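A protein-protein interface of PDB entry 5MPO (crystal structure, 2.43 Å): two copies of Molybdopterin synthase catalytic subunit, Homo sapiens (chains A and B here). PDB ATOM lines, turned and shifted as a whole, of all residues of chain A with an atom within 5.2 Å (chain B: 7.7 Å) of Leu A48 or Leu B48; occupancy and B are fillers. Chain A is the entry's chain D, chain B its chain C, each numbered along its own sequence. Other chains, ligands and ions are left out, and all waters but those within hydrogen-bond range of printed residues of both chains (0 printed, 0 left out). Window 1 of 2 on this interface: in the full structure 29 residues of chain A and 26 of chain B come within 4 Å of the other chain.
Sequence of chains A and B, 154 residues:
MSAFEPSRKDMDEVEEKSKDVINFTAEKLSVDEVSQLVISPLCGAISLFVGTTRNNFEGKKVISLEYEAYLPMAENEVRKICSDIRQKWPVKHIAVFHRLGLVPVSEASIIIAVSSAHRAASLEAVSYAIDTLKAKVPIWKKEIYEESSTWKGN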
ATOM      1  N   VAL A  31     -13.864 -15.173  20.473  1.00  0.00           N
ATOM      2  CA  VAL A  31     -12.753 -14.379  20.954  1.00  0.00           C
ATOM      3  C   VAL A  31     -12.118 -13.578  19.854  1.00  0.00           C
ATOM      4  O   VAL A  31     -11.708 -12.470  20.060  1.00  0.00           O
ATOM      5  CB  VAL A  31     -11.646 -15.244  21.563  1.00  0.00           C
ATOM      6  CG1 VAL A  31     -10.501 -14.386  22.050  1.00  0.00           C
ATOM      7  CG2 VAL A  31     -12.173 -16.060  22.709  1.00  0.00           C
ATOM      8  N   VAL A  34     -14.357 -10.601  18.710  1.00  0.00           N
ATOM      9  CA  VAL A  34     -14.268  -9.519  19.704  1.00  0.00           C
ATOM     10  C   VAL A  34     -12.913  -8.809  19.769  1.00  0.00           C
ATOM     11  O   VAL A  34     -12.881  -7.577  19.886  1.00  0.00           O
ATOM     12  CB  VAL A  34     -14.654 -10.022  21.123  1.00  0.00           C
ATOM     13  CG1 VAL A  34     -14.361  -8.971  22.212  1.00  0.00           C
ATOM     14  CG2 VAL A  34     -16.123 -10.436  21.152  1.00  0.00           C
ATOM     15  N   SER A  35     -11.802  -9.559  19.738  1.00  0.00           N
ATOM     16  CA  SER A  35     -10.452  -8.938  19.659  1.00  0.00           C
ATOM     17  C   SER A  35     -10.359  -8.012  18.462  1.00  0.00           C
ATOM     18  O   SER A  35      -9.850  -6.891  18.574  1.00  0.00           O
ATOM     19  CB  SER A  35      -9.300  -9.965  19.622  1.00  0.00           C
ATOM     20  OG  SER A  35      -9.548 -11.011  18.704  1.00  0.00           O
ATOM     21  N   ILE A  46      -3.784  -5.078  23.809  1.00  0.00           N
ATOM     22  CA  ILE A  46      -5.147  -5.485  24.000  1.00  0.00           C
ATOM     23  C   ILE A  46      -5.168  -6.515  25.134  1.00  0.00           C
ATOM     24  O   ILE A  46      -4.457  -7.486  25.090  1.00  0.00           O
ATOM     25  CB  ILE A  46      -5.742  -6.131  22.768  1.00  0.00           C
ATOM     26  CG1 ILE A  46      -5.510  -5.278  21.534  1.00  0.00           C
ATOM     27  CG2 ILE A  46      -7.220  -6.361  22.990  1.00  0.00           C
ATOM     28  CD1 ILE A  46      -6.089  -5.871  20.261  1.00  0.00           C
ATOM     29  N   SER A  47      -5.987  -6.276  26.137  1.00  0.00           N
ATOM     30  CA  SER A  47      -6.255  -7.234  27.167  1.00  0.00           C
ATOM     31  C   SER A  47      -7.655  -7.807  26.945  1.00  0.00           C
ATOM     32  O   SER A  47      -8.545  -7.106  26.510  1.00  0.00           O
ATOM     33  CB  SER A  47      -6.097  -6.570  28.537  1.00  0.00           C
ATOM     34  OG  SER A  47      -4.754  -6.110  28.707  1.00  0.00           O
ATOM     35  N   LEU A  48      -7.822  -9.104  27.198  1.00  0.00           N
ATOM     36  CA  LEU A  48      -9.105  -9.752  27.128  1.00  0.00           C
ATOM     37  C   LEU A  48      -9.388 -10.521  28.383  1.00  0.00           C
ATOM     38  O   LEU A  48      -8.460 -11.058  28.950  1.00  0.00           O
ATOM     39  CB  LEU A  48      -9.189 -10.658  25.934  1.00  0.00           C
ATOM     40  CG  LEU A  48      -9.138  -9.888  24.601  1.00  0.00           C
ATOM     41  CD1 LEU A  48      -7.810 -10.066  23.893  1.00  0.00           C
ATOM     42  CD2 LEU A  48     -10.259 -10.371  23.712  1.00  0.00           C
ATOM     43  N   PHE A  49     -10.654 -10.504  28.844  1.00  0.00           N
ATOM     44  CA  PHE A  49     -11.140 -11.472  29.848  1.00  0.00           C
ATOM     45  C   PHE A  49     -12.235 -12.276  29.175  1.00  0.00           C
ATOM     46  O   PHE A  49     -13.063 -11.712  28.440  1.00  0.00           O
ATOM     47  CB  PHE A  49     -11.657 -10.822  31.140  1.00  0.00           C
ATOM     48  CG  PHE A  49     -12.160 -11.820  32.122  1.00  0.00           C
ATOM     49  CD1 PHE A  49     -11.296 -12.487  32.931  1.00  0.00           C
ATOM     50  CD2 PHE A  49     -13.502 -12.135  32.189  1.00  0.00           C
ATOM     51  CE1 PHE A  49     -11.732 -13.495  33.791  1.00  0.00           C
ATOM     52  CE2 PHE A  49     -13.964 -13.112  33.060  1.00  0.00           C
ATOM     53  CZ  PHE A  49     -13.082 -13.803  33.868  1.00  0.00           C
ATOM     54  N   VAL A  50     -12.200 -13.591  29.391  1.00  0.00           N
ATOM     55  CA  VAL A  50     -13.192 -14.509  28.866  1.00  0.00           C
ATOM     56  C   VAL A  50     -13.653 -15.389  30.025  1.00  0.00           C
ATOM     57  O   VAL A  50     -12.848 -16.032  30.654  1.00  0.00           O
ATOM     58  CB  VAL A  50     -12.604 -15.391  27.767  1.00  0.00           C
ATOM     59  CG1 VAL A  50     -13.603 -16.452  27.269  1.00  0.00           C
ATOM     60  CG2 VAL A  50     -12.159 -14.528  26.631  1.00  0.00           C
ATOM     61  N   ILE A 111     -17.011 -12.022  27.203  1.00  0.00           N
ATOM     62  CA  ILE A 111     -15.768 -11.586  26.679  1.00  0.00           C
ATOM     63  C   ILE A 111     -15.674 -10.105  26.794  1.00  0.00           C
ATOM     64  O   ILE A 111     -16.439  -9.399  26.179  1.00  0.00           O
ATOM     65  CB  ILE A 111     -15.629 -11.917  25.195  1.00  0.00           C
ATOM     66  CG1 ILE A 111     -15.860 -13.422  24.977  1.00  0.00           C
ATOM     67  CG2 ILE A 111     -14.240 -11.492  24.723  1.00  0.00           C
ATOM     68  CD1 ILE A 111     -15.608 -13.870  23.544  1.00  0.00           C
ATOM     69  N   ILE A 112     -14.685  -9.632  27.535  1.00  0.00           N
ATOM     70  CA  ILE A 112     -14.325  -8.201  27.570  1.00  0.00           C
ATOM     71  C   ILE A 112     -12.942  -7.954  26.949  1.00  0.00           C
ATOM     72  O   ILE A 112     -12.007  -8.718  27.204  1.00  0.00           O
ATOM     73  CB  ILE A 112     -14.264  -7.715  29.004  1.00  0.00           C
ATOM     74  CG1 ILE A 112     -15.598  -7.992  29.737  1.00  0.00           C
ATOM     75  CG2 ILE A 112     -13.881  -6.250  29.026  1.00  0.00           C
ATOM     76  CD1 ILE A 112     -15.537  -7.746  31.238  1.00  0.00           C
ATOM     77  N   ALA A 113     -12.829  -6.900  26.146  1.00  0.00           N
ATOM     78  CA  ALA A 113     -11.604  -6.544  25.462  1.00  0.00           C
ATOM     79  C   ALA A 113     -11.421  -5.031  25.522  1.00  0.00           C
ATOM     80  O   ALA A 113     -12.353  -4.312  25.337  1.00  0.00           O
ATOM     81  CB  ALA A 113     -11.648  -7.021  24.027  1.00  0.00           C
ATOM     82  N   VAL A 126      -9.495  -3.846  32.025  1.00  0.00           N
ATOM     83  CA  VAL A 126     -10.166  -5.100  31.936  1.00  0.00           C
ATOM     84  C   VAL A 126     -10.537  -5.651  33.296  1.00  0.00           C
ATOM     85  O   VAL A 126     -11.631  -6.194  33.492  1.00  0.00           O
ATOM     86  CB  VAL A 126      -9.328  -6.135  31.229  1.00  0.00           C
ATOM     87  CG1 VAL A 126      -9.888  -7.500  31.514  1.00  0.00           C
ATOM     88  CG2 VAL A 126      -9.413  -5.911  29.759  1.00  0.00           C
ATOM     89  N   SER B  30      -2.707 -16.270  16.086  1.00  0.00           N
ATOM     90  CA  SER B  30      -4.160 -16.279  16.116  1.00  0.00           C
ATOM     91  C   SER B  30      -4.667 -16.261  17.581  1.00  0.00           C
ATOM     92  O   SER B  30      -4.369 -17.174  18.367  1.00  0.00           O
ATOM     93  CB  SER B  30      -4.632 -17.528  15.373  1.00  0.00           C
ATOM     94  OG  SER B  30      -5.870 -17.955  15.856  1.00  0.00           O
ATOM     95  N   VAL B  31      -5.465 -15.257  17.937  1.00  0.00           N
ATOM     96  CA  VAL B  31      -6.010 -15.167  19.277  1.00  0.00           C
ATOM     97  C   VAL B  31      -6.907 -16.369  19.504  1.00  0.00           C
ATOM     98  O   VAL B  31      -6.888 -16.958  20.576  1.00  0.00           O
ATOM     99  CB  VAL B  31      -6.828 -13.874  19.536  1.00  0.00           C
ATOM    100  CG1 VAL B  31      -7.251 -13.794  20.990  1.00  0.00           C
ATOM    101  CG2 VAL B  31      -6.026 -12.618  19.230  1.00  0.00           C
ATOM    102  N   ASP B  32      -7.667 -16.759  18.495  1.00  0.00           N
ATOM    103  CA  ASP B  32      -8.587 -17.872  18.631  1.00  0.00           C
ATOM    104  C   ASP B  32      -7.877 -19.183  18.832  1.00  0.00           C
ATOM    105  O   ASP B  32      -8.235 -19.944  19.715  1.00  0.00           O
ATOM    106  CB  ASP B  32      -9.516 -17.979  17.416  1.00  0.00           C
ATOM    107  CG  ASP B  32     -10.819 -18.680  17.757  1.00  0.00           C
ATOM    108  OD1 ASP B  32     -11.748 -17.992  18.326  1.00  0.00           O
ATOM    109  OD2 ASP B  32     -10.855 -19.918  17.484  1.00  0.00           O
ATOM    110  N   GLU B  33      -6.873 -19.438  18.006  1.00  0.00           N
ATOM    111  CA  GLU B  33      -5.983 -20.585  18.169  1.00  0.00           C
ATOM    112  C   GLU B  33      -5.501 -20.644  19.616  1.00  0.00           C
ATOM    113  O   GLU B  33      -5.689 -21.677  20.278  1.00  0.00           O
ATOM    114  CB  GLU B  33      -4.792 -20.462  17.219  1.00  0.00           C
ATOM    115  CG  GLU B  33      -3.676 -21.518  17.339  1.00  0.00           C
ATOM    116  CD  GLU B  33      -2.250 -21.055  16.904  1.00  0.00           C
ATOM    117  OE1 GLU B  33      -1.450 -21.997  16.738  1.00  0.00           O
ATOM    118  OE2 GLU B  33      -1.887 -19.813  16.763  1.00  0.00           O
ATOM    119  N   VAL B  34      -4.918 -19.532  20.112  1.00  0.00           N
ATOM    120  CA  VAL B  34      -4.184 -19.557  21.387  1.00  0.00           C
ATOM    121  C   VAL B  34      -5.158 -19.666  22.551  1.00  0.00           C
ATOM    122  O   VAL B  34      -4.873 -20.340  23.528  1.00  0.00           O
ATOM    123  CB  VAL B  34      -3.324 -18.294  21.594  1.00  0.00           C
ATOM    124  CG1 VAL B  34      -2.721 -18.230  23.001  1.00  0.00           C
ATOM    125  CG2 VAL B  34      -2.239 -18.224  20.576  1.00  0.00           C
ATOM    126  N   SER B  35      -6.301 -18.995  22.442  1.00  0.00           N
ATOM    127  CA  SER B  35      -7.300 -19.042  23.472  1.00  0.00           C
ATOM    128  C   SER B  35      -7.803 -20.482  23.580  1.00  0.00           C
ATOM    129  O   SER B  35      -8.007 -20.945  24.688  1.00  0.00           O
ATOM    130  CB  SER B  35      -8.406 -17.989  23.249  1.00  0.00           C
ATOM    131  OG  SER B  35      -9.033 -18.202  22.025  1.00  0.00           O
ATOM    132  N   GLN B  36      -7.892 -21.216  22.464  1.00  0.00           N
ATOM    133  CA  GLN B  36      -8.324 -22.651  22.485  1.00  0.00           C
ATOM    134  C   GLN B  36      -7.327 -23.571  23.149  1.00  0.00           C
ATOM    135  O   GLN B  36      -7.689 -24.604  23.680  1.00  0.00           O
ATOM    136  CB  GLN B  36      -8.637 -23.191  21.078  1.00  0.00           C
ATOM    137  N   VAL B  38      -5.811 -23.012  25.784  1.00  0.00           N
ATOM    138  CA  VAL B  38      -5.923 -22.934  27.256  1.00  0.00           C
ATOM    139  C   VAL B  38      -7.304 -23.257  27.841  1.00  0.00           C
ATOM    140  O   VAL B  38      -7.432 -23.320  29.033  1.00  0.00           O
ATOM    141  CB  VAL B  38      -5.340 -21.610  27.828  1.00  0.00           C
ATOM    142  CG1 VAL B  38      -3.927 -21.348  27.279  1.00  0.00           C
ATOM    143  CG2 VAL B  38      -6.233 -20.405  27.569  1.00  0.00           C
ATOM    144  N   ALA B  45     -12.217 -18.964  33.871  1.00  0.00           N
ATOM    145  CA  ALA B  45     -11.618 -17.676  33.450  1.00  0.00           C
ATOM    146  C   ALA B  45     -10.376 -17.865  32.555  1.00  0.00           C
ATOM    147  O   ALA B  45      -9.503 -18.664  32.858  1.00  0.00           O
ATOM    148  CB  ALA B  45     -11.258 -16.842  34.671  1.00  0.00           C
ATOM    149  N   ILE B  46     -10.330 -17.111  31.469  1.00  0.00           N
ATOM    150  CA  ILE B  46      -9.183 -17.016  30.603  1.00  0.00           C
ATOM    151  C   ILE B  46      -8.876 -15.552  30.495  1.00  0.00           C
ATOM    152  O   ILE B  46      -9.781 -14.795  30.093  1.00  0.00           O
ATOM    153  CB  ILE B  46      -9.515 -17.553  29.208  1.00  0.00           C
ATOM    154  CG1 ILE B  46      -9.882 -19.031  29.323  1.00  0.00           C
ATOM    155  CG2 ILE B  46      -8.353 -17.361  28.248  1.00  0.00           C
ATOM    156  CD1 ILE B  46     -10.268 -19.662  28.007  1.00  0.00           C
ATOM    157  N   SER B  47      -7.660 -15.137  30.896  1.00  0.00           N
ATOM    158  CA  SER B  47      -7.211 -13.780  30.571  1.00  0.00           C
ATOM    159  C   SER B  47      -6.273 -13.910  29.419  1.00  0.00           C
ATOM    160  O   SER B  47      -5.578 -14.900  29.325  1.00  0.00           O
ATOM    161  CB  SER B  47      -6.555 -13.053  31.754  1.00  0.00           C
ATOM    162  OG  SER B  47      -7.502 -12.976  32.817  1.00  0.00           O
ATOM    163  N   LEU B  48      -6.258 -12.913  28.548  1.00  0.00           N
ATOM    164  CA  LEU B  48      -5.311 -12.849  27.434  1.00  0.00           C
ATOM    165  C   LEU B  48      -4.701 -11.475  27.307  1.00  0.00           C
ATOM    166  O   LEU B  48      -5.331 -10.476  27.655  1.00  0.00           O
ATOM    167  CB  LEU B  48      -5.963 -13.195  26.098  1.00  0.00           C
ATOM    168  CG  LEU B  48      -6.498 -14.612  25.956  1.00  0.00           C
ATOM    169  CD1 LEU B  48      -7.994 -14.585  26.075  1.00  0.00           C
ATOM    170  CD2 LEU B  48      -6.141 -15.201  24.619  1.00  0.00           C
ATOM    171  N   PHE B  49      -3.437 -11.452  26.868  1.00  0.00           N
ATOM    172  CA  PHE B  49      -2.761 -10.212  26.521  1.00  0.00           C
ATOM    173  C   PHE B  49      -2.278 -10.343  25.086  1.00  0.00           C
ATOM    174  O   PHE B  49      -1.722 -11.368  24.709  1.00  0.00           O
ATOM    175  CB  PHE B  49      -1.575  -9.846  27.449  1.00  0.00           C
ATOM    176  CG  PHE B  49      -0.856  -8.604  26.972  1.00  0.00           C
ATOM    177  CD1 PHE B  49      -1.414  -7.335  27.174  1.00  0.00           C
ATOM    178  CD2 PHE B  49       0.312  -8.700  26.201  1.00  0.00           C
ATOM    179  CE1 PHE B  49      -0.778  -6.187  26.661  1.00  0.00           C
ATOM    180  CE2 PHE B  49       0.965  -7.564  25.690  1.00  0.00           C
ATOM    181  CZ  PHE B  49       0.409  -6.305  25.909  1.00  0.00           C
ATOM    182  N   VAL B  50      -2.483  -9.307  24.293  1.00  0.00           N
ATOM    183  CA  VAL B  50      -2.105  -9.336  22.887  1.00  0.00           C
ATOM    184  C   VAL B  50      -1.355  -8.063  22.647  1.00  0.00           C
ATOM    185  O   VAL B  50      -1.880  -6.981  22.951  1.00  0.00           O
ATOM    186  CB  VAL B  50      -3.312  -9.397  21.975  1.00  0.00           C
ATOM    187  CG1 VAL B  50      -2.896  -9.370  20.508  1.00  0.00           C
ATOM    188  CG2 VAL B  50      -4.157 -10.615  22.310  1.00  0.00           C
ATOM    189  N   GLY B  51      -0.113  -8.218  22.168  1.00  0.00           N
ATOM    190  CA  GLY B  51       0.798  -7.112  21.902  1.00  0.00           C
ATOM    191  C   GLY B  51       0.782  -6.931  20.394  1.00  0.00           C
ATOM    192  O   GLY B  51       0.965  -7.883  19.646  1.00  0.00           O
ATOM    193  N   ALA B  95      -0.312 -20.344  27.814  1.00  0.00           N
ATOM    194  CA  ALA B  95       0.148 -20.353  26.461  1.00  0.00           C
ATOM    195  C   ALA B  95       0.890 -19.052  26.275  1.00  0.00           C
ATOM    196  O   ALA B  95       0.398 -18.017  26.712  1.00  0.00           O
ATOM    197  CB  ALA B  95      -1.006 -20.427  25.508  1.00  0.00           C
ATOM    198  N   ILE B 111       1.071 -13.146  22.216  1.00  0.00           N
ATOM    199  CA  ILE B 111      -0.226 -13.455  22.769  1.00  0.00           C
ATOM    200  C   ILE B 111       0.125 -14.355  23.906  1.00  0.00           C
ATOM    201  O   ILE B 111       0.805 -15.380  23.736  1.00  0.00           O
ATOM    202  CB  ILE B 111      -1.162 -14.168  21.772  1.00  0.00           C
ATOM    203  CG1 ILE B 111      -1.535 -13.279  20.597  1.00  0.00           C
ATOM    204  CG2 ILE B 111      -2.463 -14.629  22.399  1.00  0.00           C
ATOM    205  CD1 ILE B 111      -2.303 -14.057  19.530  1.00  0.00           C
ATOM    206  N   ILE B 112      -0.353 -13.949  25.075  1.00  0.00           N
ATOM    207  CA  ILE B 112      -0.286 -14.713  26.315  1.00  0.00           C
ATOM    208  C   ILE B 112      -1.707 -14.977  26.776  1.00  0.00           C
ATOM    209  O   ILE B 112      -2.570 -14.075  26.759  1.00  0.00           O
ATOM    210  CB  ILE B 112       0.446 -13.923  27.397  1.00  0.00           C
ATOM    211  CG1 ILE B 112       1.898 -13.666  26.983  1.00  0.00           C
ATOM    212  CG2 ILE B 112       0.456 -14.718  28.682  1.00  0.00           C
ATOM    213  CD1 ILE B 112       2.609 -12.566  27.744  1.00  0.00           C
ATOM    214  N   ALA B 113      -1.945 -16.208  27.170  1.00  0.00           N
ATOM    215  CA  ALA B 113      -3.203 -16.611  27.710  1.00  0.00           C
ATOM    216  C   ALA B 113      -2.988 -17.505  28.954  1.00  0.00           C
ATOM    217  O   ALA B 113      -2.094 -18.338  28.959  1.00  0.00           O
ATOM    218  CB  ALA B 113      -3.982 -17.357  26.642  1.00  0.00           C
ATOM    219  N   VAL B 114      -3.847 -17.342  29.964  1.00  0.00           N
ATOM    220  CA  VAL B 114      -3.874 -18.177  31.163  1.00  0.00           C
ATOM    221  C   VAL B 114      -5.287 -18.527  31.514  1.00  0.00           C
ATOM    222  O   VAL B 114      -6.131 -17.632  31.520  1.00  0.00           O
ATOM    223  CB  VAL B 114      -3.259 -17.442  32.397  1.00  0.00           C
ATOM    224  CG1 VAL B 114      -3.246 -18.374  33.608  1.00  0.00           C
ATOM    225  CG2 VAL B 114      -1.839 -16.990  32.087  1.00  0.00           C
ATOM    226  N   SER B 115      -5.536 -19.802  31.829  1.00  0.00           N
ATOM    227  CA  SER B 115      -6.860 -20.261  32.357  1.00  0.00           C
ATOM    228  C   SER B 115      -6.769 -20.676  33.807  1.00  0.00           C
ATOM    229  O   SER B 115      -5.784 -21.236  34.225  1.00  0.00           O
ATOM    230  CB  SER B 115      -7.421 -21.455  31.554  1.00  0.00           C
ATOM    231  OG  SER B 115      -6.499 -22.556  31.541  1.00  0.00           O
ATOM    232  N   SER B 122      -5.985 -15.703  36.822  1.00  0.00           N
ATOM    233  CA  SER B 122      -5.731 -15.589  35.402  1.00  0.00           C
ATOM    234  C   SER B 122      -5.306 -14.162  35.028  1.00  0.00           C
ATOM    235  O   SER B 122      -4.372 -13.999  34.247  1.00  0.00           O
ATOM    236  CB  SER B 122      -6.944 -16.056  34.605  1.00  0.00           C
ATOM    237  OG  SER B 122      -7.882 -15.000  34.499  1.00  0.00           O
ATOM    238  N   LEU B 123      -5.928 -13.142  35.620  1.00  0.00           N
ATOM    239  CA  LEU B 123      -5.549 -11.741  35.334  1.00  0.00           C
ATOM    240  C   LEU B 123      -4.207 -11.403  35.893  1.00  0.00           C
ATOM    241  O   LEU B 123      -3.427 -10.762  35.250  1.00  0.00           O
ATOM    242  CB  LEU B 123      -6.522 -10.772  35.971  1.00  0.00           C
ATOM    243  CG  LEU B 123      -7.920 -10.796  35.336  1.00  0.00           C
ATOM    244  CD1 LEU B 123      -9.032 -10.448  36.362  1.00  0.00           C
ATOM    245  CD2 LEU B 123      -7.917  -9.854  34.118  1.00  0.00           C
ATOM    246  N   VAL B 126      -1.323 -13.248  33.944  1.00  0.00           N
ATOM    247  CA  VAL B 126      -1.075 -12.711  32.628  1.00  0.00           C
ATOM    248  C   VAL B 126      -0.247 -11.468  32.779  1.00  0.00           C
ATOM    249  O   VAL B 126       0.727 -11.229  32.042  1.00  0.00           O
ATOM    250  CB  VAL B 126      -2.371 -12.403  31.887  1.00  0.00           C
ATOM    251  CG1 VAL B 126      -2.147 -11.419  30.748  1.00  0.00           C
ATOM    252  CG2 VAL B 126      -2.923 -13.685  31.307  1.00  0.00           C
ATOM    253  N   SER B 127      -0.625 -10.683  33.758  1.00  0.00           N
ATOM    254  CA  SER B 127       0.064  -9.450  34.020  1.00  0.00           C
ATOM    255  C   SER B 127       1.539  -9.695  34.415  1.00  0.00           C
ATOM    256  O   SER B 127       2.418  -9.059  33.878  1.00  0.00           O
ATOM    257  CB  SER B 127      -0.682  -8.678  35.100  1.00  0.00           C
ATOM    258  OG  SER B 127      -0.060  -7.447  35.296  1.00  0.00           O
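N of Val A50 is in hydrogen-bond range of O of Ile B46, at 2.8 Å. The backbone carbonyl oxygen (O) of Leu B48 is in hydrogen-bond range of the backbone NH (N) of Leu A48 (2.9 Å). The backbone carbonyl oxygen of Ile A46 is in hydrogen-bond range of the backbone NH of Val B50.
OG of Ser B35 touches CG2 of Val A31, at 3.9 Å. Ser A35 touches Val B31. Ile A46 touches Phe B49. Ser A47 touches Leu B48. Ser A47 touches Phe B49 (OG to CD1, 3.9 Å). CA of Ser B47 touches O of Leu A48 (3.4 Å). Phe A49 touches Ala B45 (CE1 to CB, 3.5 Å). Phe A49 touches Ile B46 (CA to O, 3.6 Å). Phe A49 touches Ser B47. Val A50 touches Ala B45.
The backbone carbonyl oxygen of Val B31 is in hydrogen-bond range of the side-chain hydroxyl of Ser B35, 2.9 Å away. The side-chain hydroxyl (OG) of Ser B35 lies within hydrogen-bond range of the backbone carbonyl oxygen (O) of Asp B32, 3.0 Å away. OG of Ser B122 is in hydrogen-bond range of OG of Ser B47 (2.7 Å). The backbone NH of Leu B123 sits at hydrogen-bond distance from the side-chain hydroxyl of Ser B47, at 3.2 Å. The backbone NH (N) of Phe B49 is in hydrogen-bond range of the backbone carbonyl oxygen (O) of Ile B112 (2.8 Å). O of Val A31 is in hydrogen-bond range of OG of Ser A35, at 2.9 Å.
Hydrophobic or aromatic side chains of chain A that line the printed part of chain B: Val A31, Ile A46, Phe A49 and Val A50. Printed residues of chain B that touch a printed residue of chain A: Val B31, Ser B35, Ala B45, Ile B46, Ser B47, Leu B48, Phe B49 and Val B50. Along chain B the printed residues that touch a printed residue of chain A span positions 31 to 50.
Val A31 touches its own counterpart, Val B31. Val A31 touches Ser B35, and with the chains exchanged Ser A35 touches Val B31. Ile A46 touches Phe B49, and with the chains exchanged Phe A49 touches Ile B46. Ile A46 touches Val B50, and with the chains exchanged Val A50 touches Ile B46. Positions printed for both chains: 31, 34, 35, 46, 47, 48, 49, 50, 111, 112, 113 and 126. Of the 14 pairs that touch across the chains among the printed residues, 12 have their exchanged pair printed and touching as well.
Of chain A, only Ser A47 and Leu A48 come within 4 Å of Leu B48. Of the printed residues of chain B, Ser A35 touches Val B31 (3.9 Å). Of the printed residues of chain A, Val B31 touches Val A31 and Ser A35. Of the printed residues of chain B, Phe A49 touches Ala B45, Ile B46 and Ser B47. Printed residues of chain A within 4 Å of Ala B45: Phe A49 and Val A50. Of the printed residues of chain A, Ser B47 touches Leu A48 and Phe A49. Ala B95 touches none of the printed residues of chain A.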
